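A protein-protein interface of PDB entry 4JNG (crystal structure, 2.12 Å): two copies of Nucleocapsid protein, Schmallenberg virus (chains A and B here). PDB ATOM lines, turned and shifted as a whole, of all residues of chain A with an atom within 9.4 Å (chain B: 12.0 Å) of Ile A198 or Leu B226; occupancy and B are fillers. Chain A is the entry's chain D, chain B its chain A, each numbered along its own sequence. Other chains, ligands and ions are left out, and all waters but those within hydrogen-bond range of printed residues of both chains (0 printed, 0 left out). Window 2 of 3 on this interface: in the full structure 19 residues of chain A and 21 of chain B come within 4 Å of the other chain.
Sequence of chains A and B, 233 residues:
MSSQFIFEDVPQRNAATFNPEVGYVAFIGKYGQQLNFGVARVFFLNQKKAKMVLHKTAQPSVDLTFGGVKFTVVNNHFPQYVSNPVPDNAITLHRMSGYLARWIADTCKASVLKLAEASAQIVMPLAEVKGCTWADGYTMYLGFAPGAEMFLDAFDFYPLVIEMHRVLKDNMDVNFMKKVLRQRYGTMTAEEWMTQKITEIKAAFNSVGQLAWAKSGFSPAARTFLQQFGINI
No position is printed for both chains.
Among the printed residues, no Asp or Glu carboxylate lies within 4 Å of a Lys or Arg side-chain nitrogen of the other chain.
The guanidinium group of Arg B223 is in hydrogen-bond range of the side-chain sulfur of Met A164 (3.4 Å).
SD of Met A194 sits close to O of Pro B220 (3.8 Å).
Ala A190 touches none of the printed residues of chain B.
No residue of chain B comes within 4 Å of Thr A195.
No residue of chain B comes within 4 Å of Lys A197.
Ile A198 touches just these residues of chain B: Arg B223 and Leu B226.
Glu A200 touches none of the printed residues of chain B.
No residue of chain B comes within 4 Å of Lys A202.
Printed residues of chain A within 4 Å of Phe B218: Glu A191 (3.0 Å) and Met A194 (3.8 Å).
Printed residues of chain A within 4 Å of Pro B220: Met A194 (3.4 Å).
Leu B226 touches just one residue of chain A: Ile A198.
The nearest residue of chain B that does not touch Ile A198 is Gln B227 (4.1 Å).
The nearest printed residue of chain B that does not touch Ile A201 is Gln B227 (4.5 Å).
Among the printed residues, pairs that only touch across the chains: Glu A191 with Phe B218, Leu A160 with Arg B223, Met A194 with Arg B223, Ile A198 with Leu B226, Leu A168 with Gln B227, Leu A168 with Gln B228, Ile A198 with Arg B223, Phe A205 with Gln B227, Met A194 with Phe B218, Met A164 with Gln B227 and Ile A201 with Arg B223.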
ATOM      1  N   PHE A 157     -24.964 -36.768  -7.728  1.00  0.00           N
ATOM      2  CA  PHE A 157     -24.755 -35.421  -7.181  1.00  0.00           C
ATOM      3  C   PHE A 157     -25.895 -34.864  -6.296  1.00  0.00           C
ATOM      4  O   PHE A 157     -25.807 -33.726  -5.857  1.00  0.00           O
ATOM      5  CB  PHE A 157     -24.473 -34.405  -8.301  1.00  0.00           C
ATOM      6  CG  PHE A 157     -23.073 -34.452  -8.842  1.00  0.00           C
ATOM      7  CD1 PHE A 157     -22.011 -33.931  -8.113  1.00  0.00           C
ATOM      8  CD2 PHE A 157     -22.825 -34.967 -10.096  1.00  0.00           C
ATOM      9  CE1 PHE A 157     -20.725 -33.949  -8.619  1.00  0.00           C
ATOM     10  CE2 PHE A 157     -21.545 -34.989 -10.611  1.00  0.00           C
ATOM     11  CZ  PHE A 157     -20.487 -34.483  -9.873  1.00  0.00           C
ATOM     12  N   LEU A 160     -25.072 -33.210  -2.782  1.00  0.00           N
ATOM     13  CA  LEU A 160     -24.520 -31.879  -2.980  1.00  0.00           C
ATOM     14  C   LEU A 160     -25.591 -30.798  -3.182  1.00  0.00           C
ATOM     15  O   LEU A 160     -25.577 -29.793  -2.486  1.00  0.00           O
ATOM     16  CB  LEU A 160     -23.583 -31.881  -4.186  1.00  0.00           C
ATOM     17  CG  LEU A 160     -23.085 -30.524  -4.672  1.00  0.00           C
ATOM     18  CD1 LEU A 160     -22.264 -29.834  -3.592  1.00  0.00           C
ATOM     19  CD2 LEU A 160     -22.300 -30.748  -5.950  1.00  0.00           C
ATOM     20  N   MET A 164     -27.116 -27.335  -1.121  1.00  0.00           N
ATOM     21  CA  MET A 164     -27.172 -25.995  -1.718  1.00  0.00           C
ATOM     22  C   MET A 164     -28.562 -25.385  -1.477  1.00  0.00           C
ATOM     23  O   MET A 164     -28.684 -24.215  -1.106  1.00  0.00           O
ATOM     24  CB  MET A 164     -26.843 -26.044  -3.227  1.00  0.00           C
ATOM     25  CG  MET A 164     -25.458 -26.622  -3.549  1.00  0.00           C
ATOM     26  SD  MET A 164     -24.788 -26.368  -5.213  1.00  0.00           S
ATOM     27  CE  MET A 164     -25.666 -27.597  -6.178  1.00  0.00           C
ATOM     28  N   LEU A 168     -29.860 -22.180   0.745  1.00  0.00           N
ATOM     29  CA  LEU A 168     -30.592 -21.126   0.046  1.00  0.00           C
ATOM     30  C   LEU A 168     -32.005 -20.837   0.563  1.00  0.00           C
ATOM     31  O   LEU A 168     -32.387 -19.671   0.631  1.00  0.00           O
ATOM     32  CB  LEU A 168     -30.636 -21.421  -1.458  1.00  0.00           C
ATOM     33  CG  LEU A 168     -29.370 -21.006  -2.210  1.00  0.00           C
ATOM     34  CD1 LEU A 168     -29.231 -21.785  -3.508  1.00  0.00           C
ATOM     35  CD2 LEU A 168     -29.368 -19.507  -2.481  1.00  0.00           C
ATOM     36  N   TYR A 185     -15.918 -37.322  -7.036  1.00  0.00           N
ATOM     37  CA  TYR A 185     -16.914 -37.881  -7.933  1.00  0.00           C
ATOM     38  C   TYR A 185     -16.212 -38.955  -8.735  1.00  0.00           C
ATOM     39  O   TYR A 185     -15.634 -38.678  -9.789  1.00  0.00           O
ATOM     40  CB  TYR A 185     -17.500 -36.799  -8.840  1.00  0.00           C
ATOM     41  CG  TYR A 185     -18.568 -37.316  -9.773  1.00  0.00           C
ATOM     42  CD1 TYR A 185     -19.853 -37.557  -9.315  1.00  0.00           C
ATOM     43  CD2 TYR A 185     -18.289 -37.575 -11.113  1.00  0.00           C
ATOM     44  CE1 TYR A 185     -20.838 -38.030 -10.160  1.00  0.00           C
ATOM     45  CE2 TYR A 185     -19.263 -38.060 -11.967  1.00  0.00           C
ATOM     46  CZ  TYR A 185     -20.541 -38.281 -11.485  1.00  0.00           C
ATOM     47  OH  TYR A 185     -21.528 -38.753 -12.326  1.00  0.00           O
ATOM     48  N   MET A 188     -12.267 -38.280  -9.715  1.00  0.00           N
ATOM     49  CA  MET A 188     -12.141 -36.837  -9.876  1.00  0.00           C
ATOM     50  C   MET A 188     -12.175 -36.122  -8.521  1.00  0.00           C
ATOM     51  O   MET A 188     -13.075 -36.363  -7.709  1.00  0.00           O
ATOM     52  CB  MET A 188     -13.301 -36.357 -10.750  1.00  0.00           C
ATOM     53  CG  MET A 188     -13.021 -35.128 -11.583  1.00  0.00           C
ATOM     54  SD  MET A 188     -14.388 -34.632 -12.655  1.00  0.00           S
ATOM     55  CE  MET A 188     -15.087 -36.212 -13.123  1.00  0.00           C
ATOM     56  N   ALA A 190     -12.645 -32.621  -6.207  1.00  0.00           N
ATOM     57  CA  ALA A 190     -13.687 -31.591  -6.245  1.00  0.00           C
ATOM     58  C   ALA A 190     -13.365 -30.506  -7.263  1.00  0.00           C
ATOM     59  O   ALA A 190     -14.154 -30.234  -8.172  1.00  0.00           O
ATOM     60  CB  ALA A 190     -13.878 -30.982  -4.865  1.00  0.00           C
ATOM     61  N   GLU A 191     -12.190 -29.908  -7.092  1.00  0.00           N
ATOM     62  CA  GLU A 191     -11.610 -28.948  -8.034  1.00  0.00           C
ATOM     63  C   GLU A 191     -11.917 -29.267  -9.500  1.00  0.00           C
ATOM     64  O   GLU A 191     -12.094 -28.362 -10.313  1.00  0.00           O
ATOM     65  CB  GLU A 191     -10.088 -28.927  -7.842  1.00  0.00           C
ATOM     66  CG  GLU A 191      -9.439 -27.556  -7.892  1.00  0.00           C
ATOM     67  CD  GLU A 191      -8.417 -27.387  -6.784  1.00  0.00           C
ATOM     68  OE1 GLU A 191      -7.210 -27.273  -7.082  1.00  0.00           O
ATOM     69  OE2 GLU A 191      -8.827 -27.397  -5.605  1.00  0.00           O
ATOM     70  N   GLU A 192     -11.960 -30.553  -9.836  1.00  0.00           N
ATOM     71  CA  GLU A 192     -12.185 -30.966 -11.211  1.00  0.00           C
ATOM     72  C   GLU A 192     -13.666 -31.070 -11.577  1.00  0.00           C
ATOM     73  O   GLU A 192     -14.066 -30.518 -12.595  1.00  0.00           O
ATOM     74  CB  GLU A 192     -11.460 -32.279 -11.499  1.00  0.00           C
ATOM     75  CG  GLU A 192      -9.967 -32.288 -11.177  1.00  0.00           C
ATOM     76  CD  GLU A 192      -9.195 -31.121 -11.768  1.00  0.00           C
ATOM     77  OE1 GLU A 192      -9.579 -30.621 -12.849  1.00  0.00           O
ATOM     78  OE2 GLU A 192      -8.184 -30.709 -11.154  1.00  0.00           O
ATOM     79  N   TRP A 193     -14.477 -31.759 -10.771  1.00  0.00           N
ATOM     80  CA  TRP A 193     -15.922 -31.872 -11.074  1.00  0.00           C
ATOM     81  C   TRP A 193     -16.698 -30.562 -10.902  1.00  0.00           C
ATOM     82  O   TRP A 193     -17.782 -30.387 -11.484  1.00  0.00           O
ATOM     83  CB  TRP A 193     -16.618 -33.021 -10.316  1.00  0.00           C
ATOM     84  CG  TRP A 193     -16.604 -33.022  -8.784  1.00  0.00           C
ATOM     85  CD1 TRP A 193     -15.896 -33.876  -7.979  1.00  0.00           C
ATOM     86  CD2 TRP A 193     -17.379 -32.194  -7.897  1.00  0.00           C
ATOM     87  NE1 TRP A 193     -16.155 -33.609  -6.656  1.00  0.00           N
ATOM     88  CE2 TRP A 193     -17.060 -32.585  -6.575  1.00  0.00           C
ATOM     89  CE3 TRP A 193     -18.293 -31.149  -8.089  1.00  0.00           C
ATOM     90  CZ2 TRP A 193     -17.627 -31.972  -5.451  1.00  0.00           C
ATOM     91  CZ3 TRP A 193     -18.857 -30.542  -6.968  1.00  0.00           C
ATOM     92  CH2 TRP A 193     -18.516 -30.953  -5.669  1.00  0.00           C
ATOM     93  N   MET A 194     -16.159 -29.644 -10.110  1.00  0.00           N
ATOM     94  CA  MET A 194     -16.794 -28.341  -9.953  1.00  0.00           C
ATOM     95  C   MET A 194     -16.811 -27.606 -11.293  1.00  0.00           C
ATOM     96  O   MET A 194     -17.716 -26.818 -11.549  1.00  0.00           O
ATOM     97  CB  MET A 194     -16.102 -27.514  -8.870  1.00  0.00           C
ATOM     98  CG  MET A 194     -16.604 -27.840  -7.467  1.00  0.00           C
ATOM     99  SD  MET A 194     -15.836 -26.924  -6.109  1.00  0.00           S
ATOM    100  CE  MET A 194     -14.166 -26.738  -6.693  1.00  0.00           C
ATOM    101  N   THR A 195     -15.831 -27.895 -12.156  1.00  0.00           N
ATOM    102  CA  THR A 195     -15.815 -27.348 -13.512  1.00  0.00           C
ATOM    103  C   THR A 195     -16.416 -28.325 -14.517  1.00  0.00           C
ATOM    104  O   THR A 195     -17.348 -27.981 -15.249  1.00  0.00           O
ATOM    105  CB  THR A 195     -14.383 -26.993 -13.971  1.00  0.00           C
ATOM    106  OG1 THR A 195     -13.560 -28.169 -13.970  1.00  0.00           O
ATOM    107  CG2 THR A 195     -13.767 -25.943 -13.059  1.00  0.00           C
ATOM    108  N   GLN A 196     -15.879 -29.543 -14.533  1.00  0.00           N
ATOM    109  CA  GLN A 196     -16.151 -30.514 -15.594  1.00  0.00           C
ATOM    110  C   GLN A 196     -17.564 -31.079 -15.592  1.00  0.00           C
ATOM    111  O   GLN A 196     -18.042 -31.537 -16.627  1.00  0.00           O
ATOM    112  CB  GLN A 196     -15.160 -31.684 -15.519  1.00  0.00           C
ATOM    113  CG  GLN A 196     -13.719 -31.320 -15.845  1.00  0.00           C
ATOM    114  CD  GLN A 196     -12.837 -32.536 -16.076  1.00  0.00           C
ATOM    115  OE1 GLN A 196     -11.766 -32.656 -15.485  1.00  0.00           O
ATOM    116  NE2 GLN A 196     -13.281 -33.442 -16.942  1.00  0.00           N
ATOM    117  N   LYS A 197     -18.227 -31.056 -14.441  1.00  0.00           N
ATOM    118  CA  LYS A 197     -19.530 -31.705 -14.292  1.00  0.00           C
ATOM    119  C   LYS A 197     -20.650 -30.718 -13.911  1.00  0.00           C
ATOM    120  O   LYS A 197     -21.694 -31.121 -13.391  1.00  0.00           O
ATOM    121  CB  LYS A 197     -19.403 -32.826 -13.254  1.00  0.00           C
ATOM    122  CG  LYS A 197     -20.141 -34.109 -13.609  1.00  0.00           C
ATOM    123  CD  LYS A 197     -19.496 -34.894 -14.746  1.00  0.00           C
ATOM    124  CE  LYS A 197     -18.226 -35.601 -14.303  1.00  0.00           C
ATOM    125  NZ  LYS A 197     -17.987 -36.881 -15.038  1.00  0.00           N
ATOM    126  N   ILE A 198     -20.438 -29.435 -14.206  1.00  0.00           N
ATOM    127  CA  ILE A 198     -21.403 -28.370 -13.871  1.00  0.00           C
ATOM    128  C   ILE A 198     -22.786 -28.582 -14.516  1.00  0.00           C
ATOM    129  O   ILE A 198     -23.802 -28.206 -13.934  1.00  0.00           O
ATOM    130  CB  ILE A 198     -20.849 -26.966 -14.244  1.00  0.00           C
ATOM    131  CG1 ILE A 198     -21.666 -25.846 -13.586  1.00  0.00           C
ATOM    132  CG2 ILE A 198     -20.807 -26.765 -15.752  1.00  0.00           C
ATOM    133  CD1 ILE A 198     -21.288 -25.569 -12.151  1.00  0.00           C
ATOM    134  N   THR A 199     -22.818 -29.184 -15.705  1.00  0.00           N
ATOM    135  CA  THR A 199     -24.076 -29.440 -16.416  1.00  0.00           C
ATOM    136  C   THR A 199     -24.970 -30.451 -15.707  1.00  0.00           C
ATOM    137  O   THR A 199     -26.176 -30.246 -15.605  1.00  0.00           O
ATOM    138  CB  THR A 199     -23.817 -29.994 -17.828  1.00  0.00           C
ATOM    139  OG1 THR A 199     -22.932 -29.121 -18.543  1.00  0.00           O
ATOM    140  CG2 THR A 199     -25.130 -30.139 -18.594  1.00  0.00           C
ATOM    141  N   GLU A 200     -24.390 -31.567 -15.271  1.00  0.00           N
ATOM    142  CA  GLU A 200     -25.143 -32.567 -14.515  1.00  0.00           C
ATOM    143  C   GLU A 200     -25.581 -31.982 -13.181  1.00  0.00           C
ATOM    144  O   GLU A 200     -26.701 -32.216 -12.732  1.00  0.00           O
ATOM    145  CB  GLU A 200     -24.315 -33.832 -14.270  1.00  0.00           C
ATOM    146  CG  GLU A 200     -24.202 -34.762 -15.472  1.00  0.00           C
ATOM    147  CD  GLU A 200     -23.022 -34.455 -16.386  1.00  0.00           C
ATOM    148  OE1 GLU A 200     -22.398 -33.379 -16.249  1.00  0.00           O
ATOM    149  OE2 GLU A 200     -22.714 -35.304 -17.255  1.00  0.00           O
ATOM    150  N   ILE A 201     -24.688 -31.213 -12.564  1.00  0.00           N
ATOM    151  CA  ILE A 201     -24.941 -30.606 -11.260  1.00  0.00           C
ATOM    152  C   ILE A 201     -26.084 -29.585 -11.363  1.00  0.00           C
ATOM    153  O   ILE A 201     -26.973 -29.555 -10.506  1.00  0.00           O
ATOM    154  CB  ILE A 201     -23.649 -29.975 -10.688  1.00  0.00           C
ATOM    155  CG1 ILE A 201     -22.622 -31.076 -10.365  1.00  0.00           C
ATOM    156  CG2 ILE A 201     -23.936 -29.165  -9.436  1.00  0.00           C
ATOM    157  CD1 ILE A 201     -21.230 -30.558 -10.066  1.00  0.00           C
ATOM    158  N   LYS A 202     -26.066 -28.765 -12.412  1.00  0.00           N
ATOM    159  CA  LYS A 202     -27.186 -27.854 -12.687  1.00  0.00           C
ATOM    160  C   LYS A 202     -28.487 -28.629 -12.914  1.00  0.00           C
ATOM    161  O   LYS A 202     -29.539 -28.216 -12.447  1.00  0.00           O
ATOM    162  CB  LYS A 202     -26.883 -26.965 -13.896  1.00  0.00           C
ATOM    163  CG  LYS A 202     -26.113 -25.697 -13.555  1.00  0.00           C
ATOM    164  CD  LYS A 202     -25.287 -25.195 -14.734  1.00  0.00           C
ATOM    165  CE  LYS A 202     -25.454 -23.700 -14.977  1.00  0.00           C
ATOM    166  NZ  LYS A 202     -25.276 -22.863 -13.760  1.00  0.00           N
ATOM    167  N   ALA A 203     -28.407 -29.756 -13.622  1.00  0.00           N
ATOM    168  CA  ALA A 203     -29.581 -30.611 -13.845  1.00  0.00           C
ATOM    169  C   ALA A 203     -30.147 -31.144 -12.533  1.00  0.00           C
ATOM    170  O   ALA A 203     -31.351 -31.050 -12.298  1.00  0.00           O
ATOM    171  CB  ALA A 203     -29.245 -31.764 -14.781  1.00  0.00           C
ATOM    172  N   ALA A 204     -29.278 -31.695 -11.685  1.00  0.00           N
ATOM    173  CA  ALA A 204     -29.673 -32.146 -10.343  1.00  0.00           C
ATOM    174  C   ALA A 204     -30.255 -31.010  -9.489  1.00  0.00           C
ATOM    175  O   ALA A 204     -31.153 -31.235  -8.674  1.00  0.00           O
ATOM    176  CB  ALA A 204     -28.486 -32.776  -9.630  1.00  0.00           C
ATOM    177  N   PHE A 205     -29.745 -29.798  -9.688  1.00  0.00           N
ATOM    178  CA  PHE A 205     -30.195 -28.622  -8.942  1.00  0.00           C
ATOM    179  C   PHE A 205     -31.623 -28.184  -9.264  1.00  0.00           C
ATOM    180  O   PHE A 205     -32.314 -27.657  -8.397  1.00  0.00           O
ATOM    181  CB  PHE A 205     -29.220 -27.452  -9.148  1.00  0.00           C
ATOM    182  CG  PHE A 205     -29.540 -26.232  -8.317  1.00  0.00           C
ATOM    183  CD1 PHE A 205     -29.099 -26.133  -7.004  1.00  0.00           C
ATOM    184  CD2 PHE A 205     -30.275 -25.183  -8.851  1.00  0.00           C
ATOM    185  CE1 PHE A 205     -29.392 -25.016  -6.237  1.00  0.00           C
ATOM    186  CE2 PHE A 205     -30.570 -24.060  -8.091  1.00  0.00           C
ATOM    187  CZ  PHE A 205     -30.127 -23.976  -6.781  1.00  0.00           C
ATOM    188  N   ASN A 206     -32.066 -28.433 -10.491  1.00  0.00           N
ATOM    189  CA  ASN A 206     -33.234 -27.731 -11.047  1.00  0.00           C
ATOM    190  C   ASN A 206     -34.707 -27.887 -10.593  1.00  0.00           C
ATOM    191  O   ASN A 206     -35.379 -26.847 -10.612  1.00  0.00           O
ATOM    192  CB  ASN A 206     -33.165 -27.719 -12.584  1.00  0.00           C
ATOM    193  CG  ASN A 206     -32.140 -26.725 -13.112  1.00  0.00           C
ATOM    194  OD1 ASN A 206     -31.895 -25.681 -12.501  1.00  0.00           O
ATOM    195  ND2 ASN A 206     -31.531 -27.047 -14.249  1.00  0.00           N
ATOM    196  N   PHE B 218     -11.750 -21.198   0.092  1.00  0.00           N
ATOM    197  CA  PHE B 218     -11.132 -21.733  -1.139  1.00  0.00           C
ATOM    198  C   PHE B 218     -11.902 -21.490  -2.452  1.00  0.00           C
ATOM    199  O   PHE B 218     -13.129 -21.484  -2.466  1.00  0.00           O
ATOM    200  CB  PHE B 218     -10.788 -23.225  -0.930  1.00  0.00           C
ATOM    201  CG  PHE B 218     -11.017 -24.099  -2.128  1.00  0.00           C
ATOM    202  CD1 PHE B 218     -12.221 -24.768  -2.302  1.00  0.00           C
ATOM    203  CD2 PHE B 218     -10.009 -24.292  -3.050  1.00  0.00           C
ATOM    204  CE1 PHE B 218     -12.418 -25.593  -3.396  1.00  0.00           C
ATOM    205  CE2 PHE B 218     -10.197 -25.113  -4.147  1.00  0.00           C
ATOM    206  CZ  PHE B 218     -11.403 -25.765  -4.324  1.00  0.00           C
ATOM    207  N   SER B 219     -11.166 -21.296  -3.547  1.00  0.00           N
ATOM    208  CA  SER B 219     -11.770 -21.036  -4.863  1.00  0.00           C
ATOM    209  C   SER B 219     -11.665 -22.245  -5.783  1.00  0.00           C
ATOM    210  O   SER B 219     -10.568 -22.758  -5.999  1.00  0.00           O
ATOM    211  CB  SER B 219     -11.103 -19.831  -5.527  1.00  0.00           C
ATOM    212  OG  SER B 219      -9.697 -19.888  -5.408  1.00  0.00           O
ATOM    213  N   PRO B 220     -12.799 -22.724  -6.326  1.00  0.00           N
ATOM    214  CA  PRO B 220     -14.216 -22.362  -6.132  1.00  0.00           C
ATOM    215  C   PRO B 220     -14.738 -22.796  -4.761  1.00  0.00           C
ATOM    216  O   PRO B 220     -14.352 -23.889  -4.373  1.00  0.00           O
ATOM    217  CB  PRO B 220     -14.931 -23.194  -7.201  1.00  0.00           C
ATOM    218  CG  PRO B 220     -13.896 -23.590  -8.183  1.00  0.00           C
ATOM    219  CD  PRO B 220     -12.637 -23.737  -7.383  1.00  0.00           C
ATOM    220  N   ALA B 221     -15.583 -22.065  -3.997  1.00  0.00           N
ATOM    221  CA  ALA B 221     -16.136 -20.669  -4.122  1.00  0.00           C
ATOM    222  C   ALA B 221     -16.711 -20.083  -5.414  1.00  0.00           C
ATOM    223  O   ALA B 221     -17.855 -19.622  -5.413  1.00  0.00           O
ATOM    224  CB  ALA B 221     -15.228 -19.648  -3.434  1.00  0.00           C
ATOM    225  N   ALA B 222     -15.919 -20.007  -6.478  1.00  0.00           N
ATOM    226  CA  ALA B 222     -16.433 -19.734  -7.821  1.00  0.00           C
ATOM    227  C   ALA B 222     -17.638 -20.615  -8.185  1.00  0.00           C
ATOM    228  O   ALA B 222     -18.471 -20.230  -9.016  1.00  0.00           O
ATOM    229  CB  ALA B 222     -15.321 -19.904  -8.851  1.00  0.00           C
ATOM    230  N   ARG B 223     -17.747 -21.771  -7.534  1.00  0.00           N
ATOM    231  CA  ARG B 223     -18.771 -22.758  -7.851  1.00  0.00           C
ATOM    232  C   ARG B 223     -20.104 -22.354  -7.227  1.00  0.00           C
ATOM    233  O   ARG B 223     -21.114 -22.259  -7.915  1.00  0.00           O
ATOM    234  CB  ARG B 223     -18.358 -24.141  -7.328  1.00  0.00           C
ATOM    235  CG  ARG B 223     -18.680 -25.309  -8.248  1.00  0.00           C
ATOM    236  CD  ARG B 223     -20.125 -25.424  -8.692  1.00  0.00           C
ATOM    237  NE  ARG B 223     -20.823 -26.547  -8.076  1.00  0.00           N
ATOM    238  CZ  ARG B 223     -21.218 -26.599  -6.803  1.00  0.00           C
ATOM    239  NH1 ARG B 223     -20.972 -25.610  -5.953  1.00  0.00           N
ATOM    240  NH2 ARG B 223     -21.856 -27.670  -6.374  1.00  0.00           N
ATOM    241  N   THR B 224     -20.111 -22.127  -5.918  1.00  0.00           N
ATOM    242  CA  THR B 224     -21.377 -21.851  -5.229  1.00  0.00           C
ATOM    243  C   THR B 224     -21.959 -20.465  -5.547  1.00  0.00           C
ATOM    244  O   THR B 224     -23.175 -20.285  -5.487  1.00  0.00           O
ATOM    245  CB  THR B 224     -21.275 -22.050  -3.707  1.00  0.00           C
ATOM    246  OG1 THR B 224     -20.209 -21.259  -3.182  1.00  0.00           O
ATOM    247  CG2 THR B 224     -21.043 -23.519  -3.370  1.00  0.00           C
ATOM    248  N   PHE B 225     -21.101 -19.506  -5.908  1.00  0.00           N
ATOM    249  CA  PHE B 225     -21.548 -18.186  -6.397  1.00  0.00           C
ATOM    250  C   PHE B 225     -22.433 -18.353  -7.626  1.00  0.00           C
ATOM    251  O   PHE B 225     -23.399 -17.614  -7.824  1.00  0.00           O
ATOM    252  CB  PHE B 225     -20.359 -17.317  -6.812  1.00  0.00           C
ATOM    253  CG  PHE B 225     -19.509 -16.817  -5.674  1.00  0.00           C
ATOM    254  CD1 PHE B 225     -19.598 -17.337  -4.385  1.00  0.00           C
ATOM    255  CD2 PHE B 225     -18.567 -15.833  -5.919  1.00  0.00           C
ATOM    256  CE1 PHE B 225     -18.783 -16.858  -3.370  1.00  0.00           C
ATOM    257  CE2 PHE B 225     -17.757 -15.355  -4.914  1.00  0.00           C
ATOM    258  CZ  PHE B 225     -17.860 -15.863  -3.637  1.00  0.00           C
ATOM    259  N   LEU B 226     -22.067 -19.332  -8.449  1.00  0.00           N
ATOM    260  CA  LEU B 226     -22.787 -19.698  -9.669  1.00  0.00           C
ATOM    261  C   LEU B 226     -24.231 -20.133  -9.394  1.00  0.00           C
ATOM    262  O   LEU B 226     -25.066 -20.129 -10.299  1.00  0.00           O
ATOM    263  CB  LEU B 226     -22.030 -20.847 -10.352  1.00  0.00           C
ATOM    264  CG  LEU B 226     -21.951 -21.009 -11.866  1.00  0.00           C
ATOM    265  CD1 LEU B 226     -21.415 -19.756 -12.540  1.00  0.00           C
ATOM    266  CD2 LEU B 226     -21.053 -22.199 -12.180  1.00  0.00           C
ATOM    267  N   GLN B 227     -24.513 -20.508  -8.147  1.00  0.00           N
ATOM    268  CA  GLN B 227     -25.817 -21.011  -7.737  1.00  0.00           C
ATOM    269  C   GLN B 227     -26.526 -20.013  -6.802  1.00  0.00           C
ATOM    270  O   GLN B 227     -27.466 -20.377  -6.096  1.00  0.00           O
ATOM    271  CB  GLN B 227     -25.638 -22.351  -7.011  1.00  0.00           C
ATOM    272  CG  GLN B 227     -24.620 -23.313  -7.636  1.00  0.00           C
ATOM    273  CD  GLN B 227     -25.161 -24.154  -8.782  1.00  0.00           C
ATOM    274  OE1 GLN B 227     -24.387 -24.683  -9.582  1.00  0.00           O
ATOM    275  NE2 GLN B 227     -26.481 -24.294  -8.864  1.00  0.00           N
ATOM    276  N   GLN B 228     -26.065 -18.761  -6.809  1.00  0.00           N
ATOM    277  CA  GLN B 228     -26.564 -17.702  -5.922  1.00  0.00           C
ATOM    278  C   GLN B 228     -26.046 -17.840  -4.477  1.00  0.00           C
ATOM    279  O   GLN B 228     -26.694 -17.389  -3.534  1.00  0.00           O
ATOM    280  CB  GLN B 228     -28.104 -17.602  -5.967  1.00  0.00           C
ATOM    281  CG  GLN B 228     -28.657 -16.180  -5.842  1.00  0.00           C
ATOM    282  CD  GLN B 228     -29.247 -15.646  -7.143  1.00  0.00           C
ATOM    283  OE1 GLN B 228     -30.223 -16.192  -7.661  1.00  0.00           O
ATOM    284  NE2 GLN B 228     -28.670 -14.565  -7.667  1.00  0.00           N
ATOM    285  N   PHE B 229     -24.876 -18.469  -4.322  1.00  0.00           N
ATOM    286  CA  PHE B 229     -24.088 -18.411  -3.086  1.00  0.00           C
ATOM    287  C   PHE B 229     -24.728 -19.202  -1.952  1.00  0.00           C
ATOM    288  O   PHE B 229     -24.217 -20.253  -1.553  1.00  0.00           O
ATOM    289  CB  PHE B 229     -23.867 -16.939  -2.694  1.00  0.00           C
ATOM    290  CG  PHE B 229     -22.778 -16.703  -1.676  1.00  0.00           C
ATOM    291  CD1 PHE B 229     -21.686 -17.559  -1.540  1.00  0.00           C
ATOM    292  CD2 PHE B 229     -22.829 -15.568  -0.878  1.00  0.00           C
ATOM    293  CE1 PHE B 229     -20.699 -17.302  -0.601  1.00  0.00           C
ATOM    294  CE2 PHE B 229     -21.840 -15.307   0.054  1.00  0.00           C
ATOM    295  CZ  PHE B 229     -20.773 -16.174   0.192  1.00  0.00           C
